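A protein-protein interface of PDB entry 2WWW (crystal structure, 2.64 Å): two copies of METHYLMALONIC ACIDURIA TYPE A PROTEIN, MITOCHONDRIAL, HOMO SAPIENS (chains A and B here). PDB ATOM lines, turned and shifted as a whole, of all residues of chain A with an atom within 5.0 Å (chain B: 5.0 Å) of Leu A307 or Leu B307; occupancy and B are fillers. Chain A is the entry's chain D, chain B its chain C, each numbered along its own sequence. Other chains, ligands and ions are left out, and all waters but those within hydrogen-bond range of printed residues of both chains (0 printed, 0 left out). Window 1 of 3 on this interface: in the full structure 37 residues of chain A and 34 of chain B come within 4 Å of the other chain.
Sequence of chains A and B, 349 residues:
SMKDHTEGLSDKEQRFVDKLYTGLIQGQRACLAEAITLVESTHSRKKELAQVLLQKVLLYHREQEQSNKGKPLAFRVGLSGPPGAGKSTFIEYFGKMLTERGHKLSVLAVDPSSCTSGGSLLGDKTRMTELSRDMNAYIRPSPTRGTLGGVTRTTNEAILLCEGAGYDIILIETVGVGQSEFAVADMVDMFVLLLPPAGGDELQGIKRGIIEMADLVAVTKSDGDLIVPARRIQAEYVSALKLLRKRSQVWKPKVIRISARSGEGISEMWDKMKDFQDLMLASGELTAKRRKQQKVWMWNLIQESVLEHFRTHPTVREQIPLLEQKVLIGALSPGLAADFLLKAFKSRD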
ATOM      1  N   GLN A 303      17.706  15.136   8.885  1.00  0.00           N
ATOM      2  CA  GLN A 303      16.586  15.755   9.583  1.00  0.00           C
ATOM      3  C   GLN A 303      15.255  15.462   8.872  1.00  0.00           C
ATOM      4  O   GLN A 303      14.271  15.144   9.521  1.00  0.00           O
ATOM      5  CB  GLN A 303      16.834  17.262   9.638  1.00  0.00           C
ATOM      6  CG  GLN A 303      15.842  17.985  10.487  1.00  0.00           C
ATOM      7  CD  GLN A 303      16.030  19.464  10.469  1.00  0.00           C
ATOM      8  OE1 GLN A 303      16.695  20.018  11.353  1.00  0.00           O
ATOM      9  NE2 GLN A 303      15.377  20.134   9.508  1.00  0.00           N
ATOM     10  N   GLU A 304      15.217  15.574   7.553  1.00  0.00           N
ATOM     11  CA  GLU A 304      14.015  15.322   6.771  1.00  0.00           C
ATOM     12  C   GLU A 304      13.576  13.872   6.933  1.00  0.00           C
ATOM     13  O   GLU A 304      12.378  13.623   7.060  1.00  0.00           O
ATOM     14  CB  GLU A 304      14.286  15.687   5.298  1.00  0.00           C
ATOM     15  CG  GLU A 304      13.162  15.455   4.292  1.00  0.00           C
ATOM     16  CD  GLU A 304      13.619  15.143   2.868  1.00  0.00           C
ATOM     17  OE1 GLU A 304      14.829  15.279   2.546  1.00  0.00           O
ATOM     18  OE2 GLU A 304      12.747  14.695   2.084  1.00  0.00           O
ATOM     19  N   SER A 305      14.518  12.919   6.879  1.00  0.00           N
ATOM     20  CA  SER A 305      14.215  11.497   7.076  1.00  0.00           C
ATOM     21  C   SER A 305      13.829  11.231   8.530  1.00  0.00           C
ATOM     22  O   SER A 305      12.839  10.524   8.732  1.00  0.00           O
ATOM     23  CB  SER A 305      15.342  10.596   6.602  1.00  0.00           C
ATOM     24  OG  SER A 305      15.842  11.083   5.367  1.00  0.00           O
ATOM     25  N   VAL A 306      14.512  11.903   9.531  1.00  0.00           N
ATOM     26  CA  VAL A 306      14.168  11.815  10.960  1.00  0.00           C
ATOM     27  C   VAL A 306      12.676  12.221  11.163  1.00  0.00           C
ATOM     28  O   VAL A 306      11.941  11.472  11.793  1.00  0.00           O
ATOM     29  CB  VAL A 306      15.146  12.579  11.905  1.00  0.00           C
ATOM     30  CG1 VAL A 306      14.575  12.684  13.327  1.00  0.00           C
ATOM     31  CG2 VAL A 306      16.532  11.918  11.921  1.00  0.00           C
ATOM     32  N   LEU A 307      12.228  13.343  10.581  1.00  0.00           N
ATOM     33  CA  LEU A 307      10.820  13.744  10.649  1.00  0.00           C
ATOM     34  C   LEU A 307       9.853  12.856   9.886  1.00  0.00           C
ATOM     35  O   LEU A 307       8.748  12.757  10.365  1.00  0.00           O
ATOM     36  CB  LEU A 307      10.601  15.192  10.227  1.00  0.00           C
ATOM     37  CG  LEU A 307      11.309  16.218  11.088  1.00  0.00           C
ATOM     38  CD1 LEU A 307      11.513  17.491  10.327  1.00  0.00           C
ATOM     39  CD2 LEU A 307      10.530  16.475  12.351  1.00  0.00           C
ATOM     40  N   GLU A 308      10.203  12.226   8.724  1.00  0.00           N
ATOM     41  CA  GLU A 308       9.237  11.334   8.035  1.00  0.00           C
ATOM     42  C   GLU A 308       9.019  10.126   8.914  1.00  0.00           C
ATOM     43  O   GLU A 308       7.894   9.735   9.137  1.00  0.00           O
ATOM     44  CB  GLU A 308       9.712  10.833   6.647  1.00  0.00           C
ATOM     45  CG  GLU A 308      10.040  11.876   5.587  1.00  0.00           C
ATOM     46  CD  GLU A 308      10.902  11.420   4.399  1.00  0.00           C
ATOM     47  OE1 GLU A 308      11.584  12.286   3.803  1.00  0.00           O
ATOM     48  OE2 GLU A 308      10.902  10.212   4.057  1.00  0.00           O
ATOM     49  N   HIS A 309      10.107   9.554   9.440  1.00  0.00           N
ATOM     50  CA  HIS A 309      10.097   8.383  10.302  1.00  0.00           C
ATOM     51  C   HIS A 309       9.348   8.669  11.585  1.00  0.00           C
ATOM     52  O   HIS A 309       8.527   7.857  12.004  1.00  0.00           O
ATOM     53  CB  HIS A 309      11.533   7.878  10.567  1.00  0.00           C
ATOM     54  CG  HIS A 309      12.262   7.387   9.347  1.00  0.00           C
ATOM     55  ND1 HIS A 309      13.353   6.551   9.460  1.00  0.00           N
ATOM     56  CD2 HIS A 309      12.017   7.601   8.018  1.00  0.00           C
ATOM     57  CE1 HIS A 309      13.769   6.318   8.212  1.00  0.00           C
ATOM     58  NE2 HIS A 309      12.993   6.927   7.307  1.00  0.00           N
ATOM     59  N   PHE A 310       9.558   9.843  12.160  1.00  0.00           N
ATOM     60  CA  PHE A 310       8.896  10.199  13.392  1.00  0.00           C
ATOM     61  C   PHE A 310       7.385  10.448  13.204  1.00  0.00           C
ATOM     62  O   PHE A 310       6.586   9.796  13.863  1.00  0.00           O
ATOM     63  CB  PHE A 310       9.611  11.376  14.066  1.00  0.00           C
ATOM     64  CG  PHE A 310       9.087  11.737  15.438  1.00  0.00           C
ATOM     65  CD1 PHE A 310       9.604  11.130  16.580  1.00  0.00           C
ATOM     66  CD2 PHE A 310       8.114  12.727  15.593  1.00  0.00           C
ATOM     67  CE1 PHE A 310       9.148  11.494  17.851  1.00  0.00           C
ATOM     68  CE2 PHE A 310       7.640  13.070  16.862  1.00  0.00           C
ATOM     69  CZ  PHE A 310       8.160  12.449  17.982  1.00  0.00           C
ATOM     70  N   ARG A 311       7.003  11.360  12.311  1.00  0.00           N
ATOM     71  CA  ARG A 311       5.614  11.725  12.068  1.00  0.00           C
ATOM     72  C   ARG A 311       4.735  10.556  11.573  1.00  0.00           C
ATOM     73  O   ARG A 311       3.504  10.647  11.645  1.00  0.00           O
ATOM     74  CB  ARG A 311       5.520  12.977  11.145  1.00  0.00           C
ATOM     75  CG  ARG A 311       5.506  12.669   9.655  1.00  0.00           C
ATOM     76  CD  ARG A 311       5.172  13.863   8.795  1.00  0.00           C
ATOM     77  NE  ARG A 311       6.228  14.082   7.805  1.00  0.00           N
ATOM     78  CZ  ARG A 311       7.073  15.106   7.827  1.00  0.00           C
ATOM     79  NH1 ARG A 311       6.962  16.047   8.757  1.00  0.00           N
ATOM     80  NH2 ARG A 311       8.015  15.217   6.902  1.00  0.00           N
ATOM     81  N   THR A 312       5.356   9.464  11.080  1.00  0.00           N
ATOM     82  CA  THR A 312       4.618   8.300  10.585  1.00  0.00           C
ATOM     83  C   THR A 312       4.532   7.199  11.609  1.00  0.00           C
ATOM     84  O   THR A 312       3.745   6.259  11.437  1.00  0.00           O
ATOM     85  CB  THR A 312       5.138   7.818   9.220  1.00  0.00           C
ATOM     86  OG1 THR A 312       6.494   7.378   9.351  1.00  0.00           O
ATOM     87  CG2 THR A 312       4.998   8.879   8.128  1.00  0.00           C
ATOM     88  N   GLN B 303       6.744  20.296  15.521  1.00  0.00           N
ATOM     89  CA  GLN B 303       7.922  19.672  14.912  1.00  0.00           C
ATOM     90  C   GLN B 303       9.222  20.428  15.127  1.00  0.00           C
ATOM     91  O   GLN B 303      10.276  19.805  15.261  1.00  0.00           O
ATOM     92  CB  GLN B 303       7.719  19.273  13.462  1.00  0.00           C
ATOM     93  CG  GLN B 303       7.727  20.437  12.477  1.00  0.00           C
ATOM     94  CD  GLN B 303       8.025  19.937  11.089  1.00  0.00           C
ATOM     95  OE1 GLN B 303       7.519  18.891  10.648  1.00  0.00           O
ATOM     96  NE2 GLN B 303       8.879  20.658  10.378  1.00  0.00           N
ATOM     97  N   GLU B 304       9.150  21.751  15.243  1.00  0.00           N
ATOM     98  CA  GLU B 304      10.308  22.568  15.514  1.00  0.00           C
ATOM     99  C   GLU B 304      10.874  22.197  16.913  1.00  0.00           C
ATOM    100  O   GLU B 304      12.110  22.125  17.077  1.00  0.00           O
ATOM    101  CB  GLU B 304       9.895  24.051  15.480  1.00  0.00           C
ATOM    102  CG  GLU B 304      11.038  25.050  15.573  1.00  0.00           C
ATOM    103  CD  GLU B 304      10.629  26.458  15.952  1.00  0.00           C
ATOM    104  OE1 GLU B 304       9.481  26.855  15.637  1.00  0.00           O
ATOM    105  OE2 GLU B 304      11.472  27.177  16.537  1.00  0.00           O
ATOM    106  N   SER B 305       9.958  21.946  17.906  1.00  0.00           N
ATOM    107  CA  SER B 305      10.303  21.552  19.274  1.00  0.00           C
ATOM    108  C   SER B 305      10.840  20.141  19.322  1.00  0.00           C
ATOM    109  O   SER B 305      11.800  19.874  20.048  1.00  0.00           O
ATOM    110  CB  SER B 305       9.103  21.697  20.183  1.00  0.00           C
ATOM    111  OG  SER B 305       9.115  22.982  20.778  1.00  0.00           O
ATOM    112  N   VAL B 306      10.266  19.250  18.517  1.00  0.00           N
ATOM    113  CA  VAL B 306      10.720  17.857  18.382  1.00  0.00           C
ATOM    114  C   VAL B 306      12.172  17.871  17.922  1.00  0.00           C
ATOM    115  O   VAL B 306      13.003  17.229  18.558  1.00  0.00           O
ATOM    116  CB  VAL B 306       9.787  16.962  17.479  1.00  0.00           C
ATOM    117  CG1 VAL B 306      10.417  15.605  17.197  1.00  0.00           C
ATOM    118  CG2 VAL B 306       8.371  16.788  18.085  1.00  0.00           C
ATOM    119  N   LEU B 307      12.499  18.649  16.860  1.00  0.00           N
ATOM    120  CA  LEU B 307      13.888  18.748  16.357  1.00  0.00           C
ATOM    121  C   LEU B 307      14.891  19.454  17.275  1.00  0.00           C
ATOM    122  O   LEU B 307      16.049  19.059  17.221  1.00  0.00           O
ATOM    123  CB  LEU B 307      13.952  19.341  14.963  1.00  0.00           C
ATOM    124  CG  LEU B 307      13.228  18.549  13.920  1.00  0.00           C
ATOM    125  CD1 LEU B 307      12.863  19.439  12.755  1.00  0.00           C
ATOM    126  CD2 LEU B 307      14.021  17.257  13.526  1.00  0.00           C
ATOM    127  N   GLU B 308      14.499  20.495  18.089  1.00  0.00           N
ATOM    128  CA  GLU B 308      15.459  21.126  18.998  1.00  0.00           C
ATOM    129  C   GLU B 308      15.861  20.107  20.026  1.00  0.00           C
ATOM    130  O   GLU B 308      17.040  19.955  20.278  1.00  0.00           O
ATOM    131  CB  GLU B 308      14.889  22.361  19.736  1.00  0.00           C
ATOM    132  CG  GLU B 308      14.443  23.536  18.863  1.00  0.00           C
ATOM    133  CD  GLU B 308      13.553  24.595  19.511  1.00  0.00           C
ATOM    134  OE1 GLU B 308      12.740  25.224  18.791  1.00  0.00           O
ATOM    135  OE2 GLU B 308      13.680  24.811  20.740  1.00  0.00           O
ATOM    136  N   HIS B 309      14.887  19.393  20.595  1.00  0.00           N
ATOM    137  CA  HIS B 309      15.077  18.380  21.633  1.00  0.00           C
ATOM    138  C   HIS B 309      15.920  17.223  21.113  1.00  0.00           C
ATOM    139  O   HIS B 309      16.866  16.818  21.775  1.00  0.00           O
ATOM    140  CB  HIS B 309      13.731  17.890  22.204  1.00  0.00           C
ATOM    141  CG  HIS B 309      12.848  18.940  22.853  1.00  0.00           C
ATOM    142  ND1 HIS B 309      11.698  18.581  23.539  1.00  0.00           N
ATOM    143  CD2 HIS B 309      12.950  20.297  22.863  1.00  0.00           C
ATOM    144  CE1 HIS B 309      11.149  19.718  23.949  1.00  0.00           C
ATOM    145  NE2 HIS B 309      11.871  20.777  23.577  1.00  0.00           N
ATOM    146  N   PHE B 310      15.653  16.752  19.911  1.00  0.00           N
ATOM    147  CA  PHE B 310      16.376  15.686  19.242  1.00  0.00           C
ATOM    148  C   PHE B 310      17.840  16.051  18.907  1.00  0.00           C
ATOM    149  O   PHE B 310      18.751  15.275  19.235  1.00  0.00           O
ATOM    150  CB  PHE B 310      15.631  15.309  17.955  1.00  0.00           C
ATOM    151  CG  PHE B 310      16.180  14.081  17.278  1.00  0.00           C
ATOM    152  CD1 PHE B 310      15.910  12.803  17.782  1.00  0.00           C
ATOM    153  CD2 PHE B 310      16.982  14.189  16.138  1.00  0.00           C
ATOM    154  CE1 PHE B 310      16.427  11.652  17.149  1.00  0.00           C
ATOM    155  CE2 PHE B 310      17.502  13.038  15.511  1.00  0.00           C
ATOM    156  CZ  PHE B 310      17.210  11.780  16.013  1.00  0.00           C
ATOM    157  N   ARG B 311      18.073  17.196  18.204  1.00  0.00           N
ATOM    158  CA  ARG B 311      19.414  17.637  17.754  1.00  0.00           C
ATOM    159  C   ARG B 311      20.343  18.070  18.914  1.00  0.00           C
ATOM    160  O   ARG B 311      21.572  18.211  18.711  1.00  0.00           O
ATOM    161  CB  ARG B 311      19.318  18.700  16.636  1.00  0.00           C
ATOM    162  CG  ARG B 311      19.213  20.119  17.153  1.00  0.00           C
ATOM    163  CD  ARG B 311      19.346  21.176  16.075  1.00  0.00           C
ATOM    164  NE  ARG B 311      18.178  22.065  16.060  1.00  0.00           N
ATOM    165  CZ  ARG B 311      17.239  22.064  15.114  1.00  0.00           C
ATOM    166  NH1 ARG B 311      17.336  21.247  14.066  1.00  0.00           N
ATOM    167  NH2 ARG B 311      16.208  22.895  15.194  1.00  0.00           N
ATOM    168  N   THR B 312      19.773  18.265  20.131  1.00  0.00           N
ATOM    169  CA  THR B 312      20.582  18.645  21.293  1.00  0.00           C
ATOM    170  C   THR B 312      20.922  17.468  22.218  1.00  0.00           C
ATOM    171  O   THR B 312      21.826  17.578  23.042  1.00  0.00           O
ATOM    172  CB  THR B 312      19.969  19.861  22.031  1.00  0.00           C
ATOM    173  OG1 THR B 312      18.681  19.515  22.535  1.00  0.00           O
ATOM    174  CG2 THR B 312      19.897  21.126  21.156  1.00  0.00           C
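The guanidinium group (NH1) of Arg B311 lies within hydrogen-bond range of the side-chain amide oxygen (OE1) of Gln A303. The side-chain amide oxygen (OE1) of Gln B303 sits at hydrogen-bond distance from the guanidinium group (NH1) of Arg A311, 3.5 Å away.
Gln A303 touches Leu B307. Val A306 touches Phe B310 (CG1 to CE2, 3.7 Å). CD1 of Leu B307 touches CD1 of Leu A307, at 3.4 Å. CE2 of Phe A310 touches CG1 of Val B306, 3.8 Å away.
Of chain B, only Leu B307 comes within 4 Å of Leu A307. Leu B307 touches two residues of chain A. Of the printed residues of chain B, Val A306 touches Phe B310. Printed residues of chain A within 4 Å of Arg B311: Gln A303 (3.0 Å). Printed residues of chain A within 4 Å of Phe B310: Val A306. Printed residues of chain A within 4 Å of Val B306: Phe A310. Glu A308 touches none of the printed residues of chain B. The nearest residue of chain A that does not touch Leu B307 is Val A306 (4.6 Å). The nearest printed residue of chain B that does not touch Arg A311 is Val B306 (7.3 Å).
Along chain B the printed residues that touch a printed residue of chain A span positions 303 to 311. Hydrophobic or aromatic side chains of chain A that line the printed part of chain B: Val A306, Leu A307 and Phe A310. Among the printed residues, no Asp or Glu carboxylate lies within 4 Å of a Lys or Arg side-chain nitrogen of the other chain.
Gln A303 touches Leu B307, but with the chains exchanged Leu A307 does not touch Gln B303 (4.1 Å). Gln A303 touches Arg B311, and with the chains exchanged Arg A311 touches Gln B303. Val A306 touches Phe B310, and with the chains exchanged Phe A310 touches Val B306. Leu B307 touches its own counterpart, Leu A307. Positions printed for both chains: 303, 304, 305, 306, 307, 308, 309, 310, 311 and 312. Of the 6 pairs that touch across the chains among the printed residues, 5 have their exchanged pair printed and touching as well.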
